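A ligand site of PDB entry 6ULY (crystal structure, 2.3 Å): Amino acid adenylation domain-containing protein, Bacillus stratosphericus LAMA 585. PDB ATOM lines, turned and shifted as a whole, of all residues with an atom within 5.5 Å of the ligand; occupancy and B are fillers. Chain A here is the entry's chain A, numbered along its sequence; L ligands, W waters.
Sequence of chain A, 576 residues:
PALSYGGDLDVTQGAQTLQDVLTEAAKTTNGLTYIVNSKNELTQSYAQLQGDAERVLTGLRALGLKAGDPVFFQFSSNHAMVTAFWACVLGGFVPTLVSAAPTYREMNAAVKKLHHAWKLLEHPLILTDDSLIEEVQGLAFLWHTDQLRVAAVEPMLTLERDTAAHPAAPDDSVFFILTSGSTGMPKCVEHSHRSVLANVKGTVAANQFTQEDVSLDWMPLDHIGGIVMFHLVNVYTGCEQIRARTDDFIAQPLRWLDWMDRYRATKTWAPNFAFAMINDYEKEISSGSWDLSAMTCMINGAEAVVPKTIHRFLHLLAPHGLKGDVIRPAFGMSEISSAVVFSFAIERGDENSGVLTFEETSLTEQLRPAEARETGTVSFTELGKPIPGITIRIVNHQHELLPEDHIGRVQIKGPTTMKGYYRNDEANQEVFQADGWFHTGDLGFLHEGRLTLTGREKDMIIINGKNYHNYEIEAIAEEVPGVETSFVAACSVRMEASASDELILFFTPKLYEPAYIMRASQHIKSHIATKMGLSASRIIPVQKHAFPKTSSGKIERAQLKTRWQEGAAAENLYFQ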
ATOM      1  N   HIS A 223     -16.242  27.015 -10.879  1.00  0.00           N
ATOM      2  CA  HIS A 223     -15.180  27.344 -11.827  1.00  0.00           C
ATOM      3  C   HIS A 223     -14.577  26.037 -12.354  1.00  0.00           C
ATOM      4  O   HIS A 223     -14.374  25.084 -11.604  1.00  0.00           O
ATOM      5  CB  HIS A 223     -14.101  28.196 -11.152  1.00  0.00           C
ATOM      6  CG  HIS A 223     -13.126  28.821 -12.104  1.00  0.00           C
ATOM      7  ND1 HIS A 223     -12.431  28.109 -13.049  1.00  0.00           N
ATOM      8  CD2 HIS A 223     -12.724  30.112 -12.246  1.00  0.00           C
ATOM      9  CE1 HIS A 223     -11.652  28.918 -13.743  1.00  0.00           C
ATOM     10  NE2 HIS A 223     -11.820  30.147 -13.264  1.00  0.00           N
ATOM     11  N   ILE A 224     -14.314  26.010 -13.661  1.00  0.00           N
ATOM     12  CA  ILE A 224     -13.891  24.772 -14.311  1.00  0.00           C
ATOM     13  C   ILE A 224     -12.608  24.252 -13.688  1.00  0.00           C
ATOM     14  O   ILE A 224     -12.422  23.029 -13.554  1.00  0.00           O
ATOM     15  CB  ILE A 224     -13.750  24.992 -15.835  1.00  0.00           C
ATOM     16  CG1 ILE A 224     -13.669  23.643 -16.561  1.00  0.00           C
ATOM     17  CG2 ILE A 224     -12.526  25.854 -16.162  1.00  0.00           C
ATOM     18  CD1 ILE A 224     -15.013  22.959 -16.723  1.00  0.00           C
ATOM     19  N   GLY A 225     -11.701  25.149 -13.278  1.00  0.00           N
ATOM     20  CA  GLY A 225     -10.499  24.714 -12.598  1.00  0.00           C
ATOM     21  C   GLY A 225     -10.776  24.137 -11.217  1.00  0.00           C
ATOM     22  O   GLY A 225      -9.998  23.326 -10.715  1.00  0.00           O
ATOM     23  N   MET A 229      -9.929  20.691 -12.906  1.00  0.00           N
ATOM     24  CA  MET A 229      -8.477  20.718 -12.742  1.00  0.00           C
ATOM     25  C   MET A 229      -8.045  20.226 -11.368  1.00  0.00           C
ATOM     26  O   MET A 229      -6.926  19.725 -11.219  1.00  0.00           O
ATOM     27  CB  MET A 229      -7.934  22.126 -12.985  1.00  0.00           C
ATOM     28  CG  MET A 229      -6.427  22.212 -12.936  1.00  0.00           C
ATOM     29  SD  MET A 229      -5.781  23.849 -13.325  1.00  0.00           S
ATOM     30  CE  MET A 229      -6.422  24.815 -11.951  1.00  0.00           C
ATOM     31  N   TRP A 269      -4.073  26.077  -6.240  1.00  0.00           N
ATOM     32  CA  TRP A 269      -4.131  26.975  -7.384  1.00  0.00           C
ATOM     33  C   TRP A 269      -4.979  28.192  -7.057  1.00  0.00           C
ATOM     34  O   TRP A 269      -5.734  28.214  -6.080  1.00  0.00           O
ATOM     35  CB  TRP A 269      -4.702  26.276  -8.621  1.00  0.00           C
ATOM     36  CG  TRP A 269      -6.193  26.237  -8.663  1.00  0.00           C
ATOM     37  CD1 TRP A 269      -7.013  25.425  -7.943  1.00  0.00           C
ATOM     38  CD2 TRP A 269      -7.048  27.027  -9.492  1.00  0.00           C
ATOM     39  NE1 TRP A 269      -8.331  25.665  -8.263  1.00  0.00           N
ATOM     40  CE2 TRP A 269      -8.374  26.642  -9.222  1.00  0.00           C
ATOM     41  CE3 TRP A 269      -6.825  28.029 -10.444  1.00  0.00           C
ATOM     42  CZ2 TRP A 269      -9.468  27.228  -9.854  1.00  0.00           C
ATOM     43  CZ3 TRP A 269      -7.905  28.605 -11.070  1.00  0.00           C
ATOM     44  CH2 TRP A 269      -9.215  28.203 -10.777  1.00  0.00           C
ATOM     45  N   ILE A 299      -0.519  26.216  -9.032  1.00  0.00           N
ATOM     46  CA  ILE A 299      -0.957  26.567 -10.378  1.00  0.00           C
ATOM     47  C   ILE A 299      -1.531  27.977 -10.369  1.00  0.00           C
ATOM     48  O   ILE A 299      -2.344  28.341  -9.500  1.00  0.00           O
ATOM     49  CB  ILE A 299      -1.984  25.551 -10.888  1.00  0.00           C
ATOM     50  CG1 ILE A 299      -1.288  24.219 -11.198  1.00  0.00           C
ATOM     51  CG2 ILE A 299      -2.695  26.096 -12.125  1.00  0.00           C
ATOM     52  CD1 ILE A 299      -2.219  23.038 -11.288  1.00  0.00           C
ATOM     53  N   ASN A 300      -1.098  28.784 -11.322  1.00  0.00           N
ATOM     54  CA  ASN A 300      -1.546  30.165 -11.485  1.00  0.00           C
ATOM     55  C   ASN A 300      -2.202  30.280 -12.847  1.00  0.00           C
ATOM     56  O   ASN A 300      -1.521  30.260 -13.879  1.00  0.00           O
ATOM     57  CB  ASN A 300      -0.368  31.137 -11.342  1.00  0.00           C
ATOM     58  CG  ASN A 300      -0.787  32.589 -11.413  1.00  0.00           C
ATOM     59  OD1 ASN A 300      -1.887  32.904 -11.841  1.00  0.00           O
ATOM     60  ND2 ASN A 300       0.101  33.480 -11.003  1.00  0.00           N
ATOM     61  N   GLY A 301      -3.533  30.397 -12.866  1.00  0.00           N
ATOM     62  CA  GLY A 301      -4.239  30.472 -14.129  1.00  0.00           C
ATOM     63  C   GLY A 301      -5.655  30.981 -13.960  1.00  0.00           C
ATOM     64  O   GLY A 301      -6.180  31.069 -12.844  1.00  0.00           O
ATOM     65  N   ALA A 302      -6.265  31.308 -15.106  1.00  0.00           N
ATOM     66  CA  ALA A 302      -7.626  31.840 -15.242  1.00  0.00           C
ATOM     67  C   ALA A 302      -7.590  33.288 -15.727  1.00  0.00           C
ATOM     68  O   ALA A 302      -8.590  33.810 -16.234  1.00  0.00           O
ATOM     69  CB  ALA A 302      -8.439  31.749 -13.943  1.00  0.00           C
ATOM     70  N   GLU A 303      -6.447  33.943 -15.572  1.00  0.00           N
ATOM     71  CA  GLU A 303      -6.279  35.307 -16.056  1.00  0.00           C
ATOM     72  C   GLU A 303      -4.795  35.562 -16.282  1.00  0.00           C
ATOM     73  O   GLU A 303      -3.961  34.674 -16.094  1.00  0.00           O
ATOM     74  CB  GLU A 303      -6.884  36.323 -15.082  1.00  0.00           C
ATOM     75  CG  GLU A 303      -6.317  36.258 -13.666  1.00  0.00           C
ATOM     76  CD  GLU A 303      -7.013  37.233 -12.718  1.00  0.00           C
ATOM     77  OE1 GLU A 303      -6.436  37.555 -11.653  1.00  0.00           O
ATOM     78  OE2 GLU A 303      -8.134  37.674 -13.035  1.00  0.00           O
ATOM     79  N   ALA A 304      -4.477  36.786 -16.682  1.00  0.00           N
ATOM     80  CA  ALA A 304      -3.095  37.129 -17.021  1.00  0.00           C
ATOM     81  C   ALA A 304      -2.176  36.851 -15.841  1.00  0.00           C
ATOM     82  O   ALA A 304      -2.413  37.320 -14.722  1.00  0.00           O
ATOM     83  CB  ALA A 304      -3.002  38.594 -17.430  1.00  0.00           C
ATOM     84  N   VAL A 305      -1.116  36.082 -16.093  1.00  0.00           N
ATOM     85  CA  VAL A 305      -0.103  35.774 -15.103  1.00  0.00           C
ATOM     86  C   VAL A 305       0.964  36.860 -15.205  1.00  0.00           C
ATOM     87  O   VAL A 305       1.658  36.962 -16.219  1.00  0.00           O
ATOM     88  CB  VAL A 305       0.496  34.383 -15.305  1.00  0.00           C
ATOM     89  CG1 VAL A 305       1.540  34.079 -14.230  1.00  0.00           C
ATOM     90  CG2 VAL A 305      -0.603  33.330 -15.296  1.00  0.00           C
ATOM     91  N   ALA A 330      -0.709  28.477 -15.995  1.00  0.00           N
ATOM     92  CA  ALA A 330      -1.555  27.588 -16.772  1.00  0.00           C
ATOM     93  C   ALA A 330      -2.657  28.395 -17.439  1.00  0.00           C
ATOM     94  O   ALA A 330      -3.037  29.465 -16.966  1.00  0.00           O
ATOM     95  CB  ALA A 330      -2.143  26.482 -15.902  1.00  0.00           C
ATOM     96  N   PHE A 331      -3.175  27.856 -18.539  1.00  0.00           N
ATOM     97  CA  PHE A 331      -4.283  28.455 -19.261  1.00  0.00           C
ATOM     98  C   PHE A 331      -5.292  27.386 -19.643  1.00  0.00           C
ATOM     99  O   PHE A 331      -4.931  26.243 -19.926  1.00  0.00           O
ATOM    100  CB  PHE A 331      -3.820  29.201 -20.529  1.00  0.00           C
ATOM    101  CG  PHE A 331      -4.831  29.179 -21.649  1.00  0.00           C
ATOM    102  CD1 PHE A 331      -5.888  30.073 -21.661  1.00  0.00           C
ATOM    103  CD2 PHE A 331      -4.729  28.252 -22.670  1.00  0.00           C
ATOM    104  CE1 PHE A 331      -6.814  30.045 -22.685  1.00  0.00           C
ATOM    105  CE2 PHE A 331      -5.654  28.224 -23.694  1.00  0.00           C
ATOM    106  CZ  PHE A 331      -6.701  29.117 -23.697  1.00  0.00           C
ATOM    107  N   GLY A 332      -6.562  27.769 -19.646  1.00  0.00           N
ATOM    108  CA  GLY A 332      -7.601  26.856 -20.089  1.00  0.00           C
ATOM    109  C   GLY A 332      -8.920  27.585 -20.201  1.00  0.00           C
ATOM    110  O   GLY A 332      -9.009  28.799 -19.980  1.00  0.00           O
ATOM    111  N   MET A 333      -9.947  26.831 -20.556  1.00  0.00           N
ATOM    112  CA  MET A 333     -11.288  27.368 -20.692  1.00  0.00           C
ATOM    113  C   MET A 333     -12.277  26.299 -20.277  1.00  0.00           C
ATOM    114  O   MET A 333     -12.004  25.103 -20.385  1.00  0.00           O
ATOM    115  CB  MET A 333     -11.591  27.820 -22.134  1.00  0.00           C
ATOM    116  CG  MET A 333     -10.499  28.637 -22.802  1.00  0.00           C
ATOM    117  SD  MET A 333     -10.879  29.036 -24.529  1.00  0.00           S
ATOM    118  CE  MET A 333     -12.369  30.031 -24.319  1.00  0.00           C
ATOM    119  N   SER A 334     -13.452  26.744 -19.807  1.00  0.00           N
ATOM    120  CA  SER A 334     -14.511  25.794 -19.497  1.00  0.00           C
ATOM    121  C   SER A 334     -14.830  24.933 -20.705  1.00  0.00           C
ATOM    122  O   SER A 334     -15.113  23.732 -20.575  1.00  0.00           O
ATOM    123  CB  SER A 334     -15.749  26.530 -19.004  1.00  0.00           C
ATOM    124  OG  SER A 334     -16.342  27.259 -20.059  1.00  0.00           O
ATOM    125  N   GLU A 335     -14.776  25.516 -21.911  1.00  0.00           N
ATOM    126  CA  GLU A 335     -15.117  24.789 -23.125  1.00  0.00           C
ATOM    127  C   GLU A 335     -14.142  23.665 -23.441  1.00  0.00           C
ATOM    128  O   GLU A 335     -14.473  22.777 -24.232  1.00  0.00           O
ATOM    129  CB  GLU A 335     -15.181  25.738 -24.334  1.00  0.00           C
ATOM    130  CG  GLU A 335     -16.331  26.722 -24.307  1.00  0.00           C
ATOM    131  CD  GLU A 335     -15.987  28.024 -23.604  1.00  0.00           C
ATOM    132  OE1 GLU A 335     -15.054  28.031 -22.776  1.00  0.00           O
ATOM    133  OE2 GLU A 335     -16.652  29.037 -23.893  1.00  0.00           O
ATOM    134  N   SER A 338     -10.996  22.962 -18.683  1.00  0.00           N
ATOM    135  CA  SER A 338     -10.038  23.602 -17.787  1.00  0.00           C
ATOM    136  C   SER A 338      -8.666  23.686 -18.464  1.00  0.00           C
ATOM    137  O   SER A 338      -8.593  23.984 -19.662  1.00  0.00           O
ATOM    138  CB  SER A 338      -9.966  22.889 -16.413  1.00  0.00           C
ATOM    139  OG  SER A 338      -9.061  21.786 -16.381  1.00  0.00           O
ATOM    140  N   ALA A 339      -7.587  23.469 -17.719  1.00  0.00           N
ATOM    141  CA  ALA A 339      -6.266  23.807 -18.237  1.00  0.00           C
ATOM    142  C   ALA A 339      -5.828  22.849 -19.328  1.00  0.00           C
ATOM    143  O   ALA A 339      -6.112  21.649 -19.273  1.00  0.00           O
ATOM    144  CB  ALA A 339      -5.246  23.801 -17.098  1.00  0.00           C
ATOM    145  N   LEU A 383       3.092  30.062 -20.692  1.00  0.00           N
ATOM    146  CA  LEU A 383       2.099  29.169 -20.115  1.00  0.00           C
ATOM    147  C   LEU A 383       2.375  27.705 -20.435  1.00  0.00           C
ATOM    148  O   LEU A 383       1.638  26.833 -19.971  1.00  0.00           O
ATOM    149  CB  LEU A 383       0.699  29.564 -20.577  1.00  0.00           C
ATOM    150  CG  LEU A 383       0.328  31.030 -20.276  1.00  0.00           C
ATOM    151  CD1 LEU A 383      -1.111  31.321 -20.667  1.00  0.00           C
ATOM    152  CD2 LEU A 383       0.563  31.372 -18.805  1.00  0.00           C
ATOM    153  N   THR A 440     -10.677  30.019 -29.406  1.00  0.00           N
ATOM    154  CA  THR A 440     -10.700  30.439 -28.009  1.00  0.00           C
ATOM    155  C   THR A 440     -11.138  31.886 -27.839  1.00  0.00           C
ATOM    156  O   THR A 440     -11.711  32.224 -26.796  1.00  0.00           O
ATOM    157  CB  THR A 440      -9.311  30.274 -27.382  1.00  0.00           C
ATOM    158  OG1 THR A 440      -8.383  31.142 -28.050  1.00  0.00           O
ATOM    159  CG2 THR A 440      -8.833  28.833 -27.490  1.00  0.00           C
ATOM    160  N   ASP A 442      -8.796  34.066 -27.671  1.00  0.00           N
ATOM    161  CA  ASP A 442      -7.604  34.600 -27.027  1.00  0.00           C
ATOM    162  C   ASP A 442      -6.514  34.840 -28.060  1.00  0.00           C
ATOM    163  O   ASP A 442      -6.438  34.158 -29.082  1.00  0.00           O
ATOM    164  CB  ASP A 442      -7.091  33.630 -25.954  1.00  0.00           C
ATOM    165  CG  ASP A 442      -8.083  33.445 -24.824  1.00  0.00           C
ATOM    166  OD1 ASP A 442      -8.594  34.466 -24.310  1.00  0.00           O
ATOM    167  OD2 ASP A 442      -8.350  32.289 -24.457  1.00  0.00           O
ATOM    168  N   LEU A 453      -0.067  33.652 -23.883  1.00  0.00           N
ATOM    169  CA  LEU A 453      -1.198  34.514 -24.172  1.00  0.00           C
ATOM    170  C   LEU A 453      -0.789  35.976 -24.035  1.00  0.00           C
ATOM    171  O   LEU A 453      -0.027  36.345 -23.139  1.00  0.00           O
ATOM    172  CB  LEU A 453      -2.372  34.210 -23.232  1.00  0.00           C
ATOM    173  CG  LEU A 453      -3.458  33.281 -23.796  1.00  0.00           C
ATOM    174  CD1 LEU A 453      -2.863  32.130 -24.563  1.00  0.00           C
ATOM    175  CD2 LEU A 453      -4.332  32.763 -22.659  1.00  0.00           C
ATOM    176  N   ARG A 456      -6.914  39.307 -25.856  1.00  0.00           N
ATOM    177  CA  ARG A 456      -8.163  38.716 -26.298  1.00  0.00           C
ATOM    178  C   ARG A 456      -8.681  39.475 -27.514  1.00  0.00           C
ATOM    179  O   ARG A 456      -8.332  40.637 -27.736  1.00  0.00           O
ATOM    180  CB  ARG A 456      -9.228  38.756 -25.182  1.00  0.00           C
ATOM    181  CG  ARG A 456      -8.900  37.903 -23.969  1.00  0.00           C
ATOM    182  CD  ARG A 456      -9.967  38.044 -22.898  1.00  0.00           C
ATOM    183  NE  ARG A 456     -10.025  39.418 -22.383  1.00  0.00           N
ATOM    184  CZ  ARG A 456     -10.969  39.865 -21.561  1.00  0.00           C
ATOM    185  NH1 ARG A 456     -11.942  39.070 -21.152  1.00  0.00           N
ATOM    186  NH2 ARG A 456     -10.927  41.126 -21.151  1.00  0.00           N
HETATM  187  C1  LIG L   1      -6.183  27.171 -15.802  1.00  0.00           C
HETATM  188  C2  LIG L   1      -7.609  27.351 -15.432  1.00  0.00           C
HETATM  189  C3  LIG L   1      -8.260  26.021 -15.207  1.00  0.00           C
HETATM  190  C4  LIG L   1      -8.171  28.244 -16.498  1.00  0.00           C
HETATM  191  C5  LIG L   1      -9.556  27.946 -16.993  1.00  0.00           C
HETATM  192  C6  LIG L   1     -10.567  29.052 -17.032  1.00  0.00           C
HETATM  193  C7  LIG L   1     -11.345  31.070 -19.737  1.00  0.00           C
HETATM  194  C8  LIG L   1     -10.756  32.239 -20.153  1.00  0.00           C
HETATM  195  C9  LIG L   1      -9.764  31.940 -21.357  1.00  0.00           C
HETATM  196  C10 LIG L   1      -8.915  32.822 -21.274  1.00  0.00           C
HETATM  197  C11 LIG L   1      -8.815  33.253 -19.692  1.00  0.00           C
HETATM  198  C12 LIG L   1      -7.522  31.596 -18.579  1.00  0.00           C
HETATM  199  C13 LIG L   1      -5.574  32.462 -18.609  1.00  0.00           C
HETATM  200  C14 LIG L   1      -4.239  32.821 -18.497  1.00  0.00           C
HETATM  201  C15 LIG L   1      -4.649  34.733 -19.567  1.00  0.00           C
HETATM  202  C16 LIG L   1      -6.394  33.307 -19.211  1.00  0.00           C
HETATM  203  N1  LIG L   1      -7.610  32.745 -19.174  1.00  0.00           N
HETATM  204  N2  LIG L   1      -6.281  31.399 -18.230  1.00  0.00           N
HETATM  205  N3  LIG L   1      -3.823  33.936 -18.989  1.00  0.00           N
HETATM  206  N4  LIG L   1      -5.893  34.455 -19.690  1.00  0.00           N
HETATM  207  N5  LIG L   1      -3.345  31.940 -17.865  1.00  0.00           N
HETATM  208  O1  LIG L   1     -11.786  28.890 -17.580  1.00  0.00           O
HETATM  209  O2  LIG L   1     -12.241  31.268 -18.720  1.00  0.00           O
HETATM  210  O3  LIG L   1      -9.816  32.771 -19.114  1.00  0.00           O
HETATM  211  O4  LIG L   1      -9.233  34.063 -21.930  1.00  0.00           O
HETATM  212  O5  LIG L   1     -10.373  31.844 -22.727  1.00  0.00           O
HETATM  213  O6  LIG L   1     -13.575  30.288 -16.818  1.00  0.00           O
HETATM  214  O7  LIG L   1     -13.746  29.426 -18.880  1.00  0.00           O
HETATM  215  O8  LIG L   1     -10.287  30.034 -16.576  1.00  0.00           O
HETATM  216  O9  LIG L   1      -9.797  26.909 -17.379  1.00  0.00           O
HETATM  217  P1  LIG L   1     -12.832  30.009 -17.991  1.00  0.00           P
HETATM  218  O   HOH W   1     -15.049  28.246 -15.327  1.00  0.00           O
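The side-chain hydroxyl (OG1) of Thr 440 sits at hydrogen-bond distance from the backbone NH (N) of Asp 442 (3.0 Å). The backbone carbonyl oxygen of Ile 224 lies within hydrogen-bond range of the backbone NH of Met 229 (3.5 Å). The backbone NH (N) of Ala 330 is in hydrogen-bond range of the backbone carbonyl oxygen (O) of Asn 300, at 2.9 Å. O of Met 333 is in hydrogen-bond range of N of Ser 338. The side-chain hydroxyl (OG) of Ser 334 is in hydrogen-bond range of the side-chain carboxylate (OE1) of Glu 335 (3.1 Å). ND1 of His 223 lies within hydrogen-bond range of N of Gly 225, at 3.1 Å.
Water W1 lies within hydrogen-bond range of N of Ile 224, O6 of the ligand and ND1 of His 223.
O9 of the ligand lies close to O of Gly 332, at 3.3 Å. His 223 touches the ligand. CG2 of Ile 224 touches O9 of the ligand, 3.2 Å away. Gly 225 touches the ligand. SD of Met 229 touches C3 of the ligand, 3.8 Å away. Ala 304 touches the ligand. Phe 331 touches the ligand (CD1 to N2, 3.7 Å). CA of Ser 338 touches O9 of the ligand (3.3 Å). Ala 339 touches the ligand. CD1 of Leu 383 touches N5 of the ligand, at 3.6 Å. CD2 of Leu 453 touches C15 of the ligand (3.7 Å). Hydrophobic or aromatic side chains that line the ligand: His 223, Ile 224, Met 229, Ala 302, Phe 331, Met 333, Ala 339, Leu 383 and Leu 453. Of the 25 residues printed, 17 come within 4 Å of the ligand. Along chain A the residues within 4 Å of the ligand span positions 223 to 453. The nearest printed residue that does not touch the ligand is Val 305 (4.01 Å).
SD of Met 333 lies close to O5 of the ligand (3.4 Å). The side-chain carboxylate (OD1) of Asp 442 lies within hydrogen-bond range of an oxygen (O4) of the ligand (2.5 Å). N2 of the ligand sits at hydrogen-bond distance from N of Ala 302, 3.1 Å away. O of Ala 330 sits at hydrogen-bond distance from N5 of the ligand (2.7 Å). N of Met 333 sits at hydrogen-bond distance from O9 of the ligand (3.2 Å). A nitrogen (N5) of the ligand sits close to the backbone carbonyl oxygen (O) of Glu 303 (3.3 Å). The backbone NH (N) of Ser 334 sits at hydrogen-bond distance from an oxygen (O7) of the ligand (2.9 Å).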
